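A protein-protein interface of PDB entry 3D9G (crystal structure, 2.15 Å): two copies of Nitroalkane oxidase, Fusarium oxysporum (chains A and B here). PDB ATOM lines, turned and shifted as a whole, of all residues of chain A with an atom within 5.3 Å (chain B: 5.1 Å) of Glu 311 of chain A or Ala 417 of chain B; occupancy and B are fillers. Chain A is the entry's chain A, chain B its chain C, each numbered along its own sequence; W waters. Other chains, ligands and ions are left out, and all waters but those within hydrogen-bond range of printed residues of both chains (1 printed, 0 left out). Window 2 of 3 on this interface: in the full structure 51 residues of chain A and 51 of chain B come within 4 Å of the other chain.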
ATOM      1  N   LYS A 299      27.131 -19.187  33.669  1.00  0.00           N
ATOM      2  CA  LYS A 299      28.333 -20.002  33.553  1.00  0.00           C
ATOM      3  C   LYS A 299      28.640 -20.846  34.808  1.00  0.00           C
ATOM      4  O   LYS A 299      29.595 -21.613  34.817  1.00  0.00           O
ATOM      5  CB  LYS A 299      29.523 -19.106  33.206  1.00  0.00           C
ATOM      6  CG  LYS A 299      29.413 -18.437  31.828  1.00  0.00           C
ATOM      7  CD  LYS A 299      30.588 -17.491  31.560  1.00  0.00           C
ATOM      8  CE  LYS A 299      31.881 -18.293  31.516  1.00  0.00           C
ATOM      9  NZ  LYS A 299      32.830 -17.752  30.540  1.00  0.00           N
ATOM     10  N   LYS A 307      23.721 -29.353  32.981  1.00  0.00           N
ATOM     11  CA  LYS A 307      24.733 -28.463  32.401  1.00  0.00           C
ATOM     12  C   LYS A 307      24.457 -27.011  32.726  1.00  0.00           C
ATOM     13  O   LYS A 307      23.304 -26.639  32.973  1.00  0.00           O
ATOM     14  CB  LYS A 307      24.848 -28.666  30.886  1.00  0.00           C
ATOM     15  CG  LYS A 307      23.708 -28.096  30.049  1.00  0.00           C
ATOM     16  CD  LYS A 307      23.727 -28.742  28.647  1.00  0.00           C
ATOM     17  CE  LYS A 307      22.507 -28.332  27.812  1.00  0.00           C
ATOM     18  NZ  LYS A 307      22.735 -28.455  26.333  1.00  0.00           N
ATOM     19  N   HIS A 308      25.517 -26.204  32.724  1.00  0.00           N
ATOM     20  CA  HIS A 308      25.382 -24.761  32.906  1.00  0.00           C
ATOM     21  C   HIS A 308      24.390 -24.201  31.893  1.00  0.00           C
ATOM     22  O   HIS A 308      24.376 -24.598  30.705  1.00  0.00           O
ATOM     23  CB  HIS A 308      26.727 -24.043  32.757  1.00  0.00           C
ATOM     24  CG  HIS A 308      27.775 -24.485  33.736  1.00  0.00           C
ATOM     25  ND1 HIS A 308      27.484 -24.863  35.032  1.00  0.00           N
ATOM     26  CD2 HIS A 308      29.122 -24.579  33.613  1.00  0.00           C
ATOM     27  CE1 HIS A 308      28.605 -25.182  35.657  1.00  0.00           C
ATOM     28  NE2 HIS A 308      29.611 -25.028  34.815  1.00  0.00           N
ATOM     29  N   ILE A 309      23.574 -23.267  32.358  1.00  0.00           N
ATOM     30  CA  ILE A 309      22.483 -22.767  31.530  1.00  0.00           C
ATOM     31  C   ILE A 309      22.948 -22.001  30.271  1.00  0.00           C
ATOM     32  O   ILE A 309      22.220 -21.921  29.280  1.00  0.00           O
ATOM     33  CB  ILE A 309      21.391 -22.015  32.352  1.00  0.00           C
ATOM     34  CG1 ILE A 309      21.958 -20.766  33.055  1.00  0.00           C
ATOM     35  CG2 ILE A 309      20.738 -22.954  33.346  1.00  0.00           C
ATOM     36  CD1 ILE A 309      20.851 -19.800  33.560  1.00  0.00           C
ATOM     37  N   ILE A 310      24.173 -21.487  30.288  1.00  0.00           N
ATOM     38  CA  ILE A 310      24.738 -20.856  29.088  1.00  0.00           C
ATOM     39  C   ILE A 310      24.817 -21.843  27.898  1.00  0.00           C
ATOM     40  O   ILE A 310      25.016 -21.439  26.745  1.00  0.00           O
ATOM     41  CB  ILE A 310      26.142 -20.212  29.363  1.00  0.00           C
ATOM     42  CG1 ILE A 310      26.495 -19.249  28.220  1.00  0.00           C
ATOM     43  CG2 ILE A 310      27.236 -21.306  29.623  1.00  0.00           C
ATOM     44  CD1 ILE A 310      27.621 -18.301  28.483  1.00  0.00           C
ATOM     45  N   GLU A 311      24.678 -23.135  28.190  1.00  0.00           N
ATOM     46  CA  GLU A 311      24.668 -24.162  27.167  1.00  0.00           C
ATOM     47  C   GLU A 311      23.294 -24.363  26.545  1.00  0.00           C
ATOM     48  O   GLU A 311      23.146 -25.192  25.660  1.00  0.00           O
ATOM     49  CB  GLU A 311      25.213 -25.502  27.705  1.00  0.00           C
ATOM     50  CG  GLU A 311      26.693 -25.480  28.111  1.00  0.00           C
ATOM     51  CD  GLU A 311      27.655 -25.252  26.951  1.00  0.00           C
ATOM     52  OE1 GLU A 311      28.798 -24.815  27.213  1.00  0.00           O
ATOM     53  OE2 GLU A 311      27.294 -25.513  25.777  1.00  0.00           O
ATOM     54  N   HIS A 312      22.294 -23.623  27.006  1.00  0.00           N
ATOM     55  CA  HIS A 312      20.978 -23.630  26.370  1.00  0.00           C
ATOM     56  C   HIS A 312      20.920 -22.498  25.348  1.00  0.00           C
ATOM     57  O   HIS A 312      21.234 -21.360  25.671  1.00  0.00           O
ATOM     58  CB  HIS A 312      19.877 -23.447  27.414  1.00  0.00           C
ATOM     59  CG  HIS A 312      19.839 -24.533  28.441  1.00  0.00           C
ATOM     60  ND1 HIS A 312      19.667 -25.862  28.110  1.00  0.00           N
ATOM     61  CD2 HIS A 312      19.930 -24.490  29.789  1.00  0.00           C
ATOM     62  CE1 HIS A 312      19.677 -26.593  29.209  1.00  0.00           C
ATOM     63  NE2 HIS A 312      19.829 -25.786  30.243  1.00  0.00           N
ATOM     64  N   GLN A 313      20.523 -22.812  24.118  1.00  0.00           N
ATOM     65  CA  GLN A 313      20.582 -21.818  23.038  1.00  0.00           C
ATOM     66  C   GLN A 313      19.781 -20.549  23.341  1.00  0.00           C
ATOM     67  O   GLN A 313      20.234 -19.452  23.013  1.00  0.00           O
ATOM     68  CB  GLN A 313      20.154 -22.435  21.698  1.00  0.00           C
ATOM     69  CG  GLN A 313      21.193 -23.415  21.122  1.00  0.00           C
ATOM     70  CD  GLN A 313      20.859 -23.858  19.707  1.00  0.00           C
ATOM     71  OE1 GLN A 313      19.767 -23.595  19.209  1.00  0.00           O
ATOM     72  NE2 GLN A 313      21.792 -24.536  19.063  1.00  0.00           N
ATOM     73  N   MET B 412      29.671 -17.919  18.584  1.00  0.00           N
ATOM     74  CA  MET B 412      29.761 -16.963  19.705  1.00  0.00           C
ATOM     75  C   MET B 412      29.439 -17.592  21.080  1.00  0.00           C
ATOM     76  O   MET B 412      30.184 -17.390  22.040  1.00  0.00           O
ATOM     77  CB  MET B 412      28.882 -15.740  19.454  1.00  0.00           C
ATOM     78  CG  MET B 412      29.075 -14.633  20.464  1.00  0.00           C
ATOM     79  SD  MET B 412      28.293 -13.110  19.939  1.00  0.00           S
ATOM     80  CE  MET B 412      28.402 -12.145  21.469  1.00  0.00           C
ATOM     81  N   GLN B 413      28.344 -18.348  21.153  1.00  0.00           N
ATOM     82  CA  GLN B 413      27.966 -19.088  22.363  1.00  0.00           C
ATOM     83  C   GLN B 413      29.127 -19.939  22.898  1.00  0.00           C
ATOM     84  O   GLN B 413      29.392 -19.940  24.094  1.00  0.00           O
ATOM     85  CB  GLN B 413      26.732 -19.962  22.096  1.00  0.00           C
ATOM     86  CG  GLN B 413      26.245 -20.851  23.280  1.00  0.00           C
ATOM     87  CD  GLN B 413      24.958 -21.681  22.956  1.00  0.00           C
ATOM     88  OE1 GLN B 413      24.373 -21.581  21.858  1.00  0.00           O
ATOM     89  NE2 GLN B 413      24.513 -22.474  23.934  1.00  0.00           N
ATOM     90  N   ARG B 414      29.813 -20.644  22.000  1.00  0.00           N
ATOM     91  CA  ARG B 414      30.897 -21.555  22.348  1.00  0.00           C
ATOM     92  C   ARG B 414      32.044 -20.803  23.042  1.00  0.00           C
ATOM     93  O   ARG B 414      32.563 -21.257  24.053  1.00  0.00           O
ATOM     94  CB  ARG B 414      31.369 -22.258  21.070  1.00  0.00           C
ATOM     95  CG  ARG B 414      32.077 -23.591  21.242  1.00  0.00           C
ATOM     96  CD  ARG B 414      32.116 -24.368  19.899  1.00  0.00           C
ATOM     97  NE  ARG B 414      30.778 -24.892  19.554  1.00  0.00           N
ATOM     98  CZ  ARG B 414      30.064 -24.575  18.462  1.00  0.00           C
ATOM     99  NH1 ARG B 414      30.546 -23.741  17.531  1.00  0.00           N
ATOM    100  NH2 ARG B 414      28.855 -25.116  18.302  1.00  0.00           N
ATOM    101  N   VAL B 415      32.407 -19.639  22.499  1.00  0.00           N
ATOM    102  CA  VAL B 415      33.464 -18.774  23.043  1.00  0.00           C
ATOM    103  C   VAL B 415      33.059 -18.195  24.416  1.00  0.00           C
ATOM    104  O   VAL B 415      33.871 -18.157  25.351  1.00  0.00           O
ATOM    105  CB  VAL B 415      33.808 -17.624  22.042  1.00  0.00           C
ATOM    106  CG1 VAL B 415      34.624 -16.522  22.716  1.00  0.00           C
ATOM    107  CG2 VAL B 415      34.556 -18.171  20.838  1.00  0.00           C
ATOM    108  N   MET B 416      31.798 -17.768  24.526  1.00  0.00           N
ATOM    109  CA  MET B 416      31.273 -17.186  25.765  1.00  0.00           C
ATOM    110  C   MET B 416      31.239 -18.218  26.893  1.00  0.00           C
ATOM    111  O   MET B 416      31.283 -17.854  28.074  1.00  0.00           O
ATOM    112  CB  MET B 416      29.872 -16.588  25.547  1.00  0.00           C
ATOM    113  CG  MET B 416      29.822 -15.394  24.592  1.00  0.00           C
ATOM    114  SD  MET B 416      28.133 -14.783  24.307  1.00  0.00           S
ATOM    115  CE  MET B 416      27.908 -13.653  25.689  1.00  0.00           C
ATOM    116  N   ALA B 417      31.164 -19.495  26.523  1.00  0.00           N
ATOM    117  CA  ALA B 417      31.020 -20.578  27.488  1.00  0.00           C
ATOM    118  C   ALA B 417      32.356 -21.043  28.062  1.00  0.00           C
ATOM    119  O   ALA B 417      32.376 -21.762  29.049  1.00  0.00           O
ATOM    120  CB  ALA B 417      30.264 -21.755  26.870  1.00  0.00           C
ATOM    121  N   LEU B 418      33.458 -20.633  27.431  1.00  0.00           N
ATOM    122  CA  LEU B 418      34.807 -20.997  27.869  1.00  0.00           C
ATOM    123  C   LEU B 418      35.154 -20.371  29.213  1.00  0.00           C
ATOM    124  O   LEU B 418      34.821 -19.209  29.476  1.00  0.00           O
ATOM    125  CB  LEU B 418      35.853 -20.584  26.821  1.00  0.00           C
ATOM    126  CG  LEU B 418      35.793 -21.255  25.438  1.00  0.00           C
ATOM    127  CD1 LEU B 418      36.755 -20.596  24.475  1.00  0.00           C
ATOM    128  CD2 LEU B 418      36.046 -22.763  25.518  1.00  0.00           C
ATOM    129  N   GLU B 419      35.846 -21.143  30.052  1.00  0.00           N
ATOM    130  CA  GLU B 419      36.175 -20.709  31.408  1.00  0.00           C
ATOM    131  C   GLU B 419      36.965 -19.418  31.410  1.00  0.00           C
ATOM    132  O   GLU B 419      36.738 -18.559  32.248  1.00  0.00           O
ATOM    133  CB  GLU B 419      36.933 -21.796  32.177  1.00  0.00           C
ATOM    134  CG  GLU B 419      36.050 -22.654  33.055  1.00  0.00           C
ATOM    135  CD  GLU B 419      36.822 -23.365  34.175  1.00  0.00           C
ATOM    136  OE1 GLU B 419      38.081 -23.266  34.204  1.00  0.00           O
ATOM    137  OE2 GLU B 419      36.156 -24.019  35.031  1.00  0.00           O
HETATM  138  O   HOH W   1      23.375 -25.607  23.004  1.00  0.00           O
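Glu 311 of chain A touches just these residues of chain B: Gln 413 and Ala 417. Of the printed residues of chain A, Ala 417 of chain B touches Glu 311 (3.4 Å). Of the printed residues of chain B, Gln 313 of chain A touches Gln 413 (3.7 Å). Printed residues of chain A within 4 Å of Met 416 of chain B: Lys 299 and Ile 310. Of the printed residues of chain A, Gln 413 of chain B touches Ile 310 (3.0 Å), Glu 311 (3.4 Å), His 312 (3.9 Å) and Gln 313 (3.7 Å). Printed residues of chain B within 4 Å of Lys 299 of chain A: Met 416 (2.9 Å) and Leu 418 (2.7 Å). Lys 307 of chain A touches none of the printed residues of chain B. Val 415 of chain B touches none of the printed residues of chain A. The nearest printed residue of chain B that does not touch Glu 311 of chain A is Arg 414 of chain B (6.1 Å).
O of Met 416 of chain B lies within hydrogen-bond range of NZ of Lys 299 of chain A, 2.9 Å away. The side-chain amino group (NZ) of Lys 299 of chain A lies within hydrogen-bond range of the backbone carbonyl oxygen (O) of Leu 418 of chain B, 2.7 Å away. The side-chain amide nitrogen of Gln 413 of chain B sits at hydrogen-bond distance from the backbone carbonyl oxygen of Ile 310 of chain A, at 3.0 Å. O of Glu 311 of chain A lies close to NE2 of Gln 413 of chain B (3.5 Å).
The backbone carbonyl oxygen (O) of Lys 299 of chain A sits close to a ring nitrogen (NE2) of His 308 of chain A (3.4 Å). The backbone carbonyl oxygen (O) of Glu 311 of chain A lies within hydrogen-bond range of the side-chain amino group (NZ) of Lys 307 of chain A (3.4 Å).
No position is printed for both chains. Of the 8 pairs that touch across the chains among the printed residues, none has its exchanged pair printed and touching as well.
Water W1 lies within hydrogen-bond range of the backbone carbonyl oxygen (O) of Glu 311 of chain A (2.7 Å) and the side-chain amide nitrogen (NE2) of Gln 413 of chain B (3.5 Å).
O of Met 416 of chain B touches CD1 of Ile 310 of chain A (3.7 Å). CB of Ala 417 of chain B touches OE1 of Glu 311 of chain A (3.4 Å). NE2 of Gln 413 of chain B touches C of His 312 of chain A (3.9 Å). Gln 313 of chain A touches Gln 413 of chain B.
Of the 8 printed residues of chain A, 5 touch a printed residue of chain B. Hydrophobic or aromatic side chains of chain A within 4 Å of the printed part of chain B: Ile 310. Among the printed residues, 8 pairs touch across the chains.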
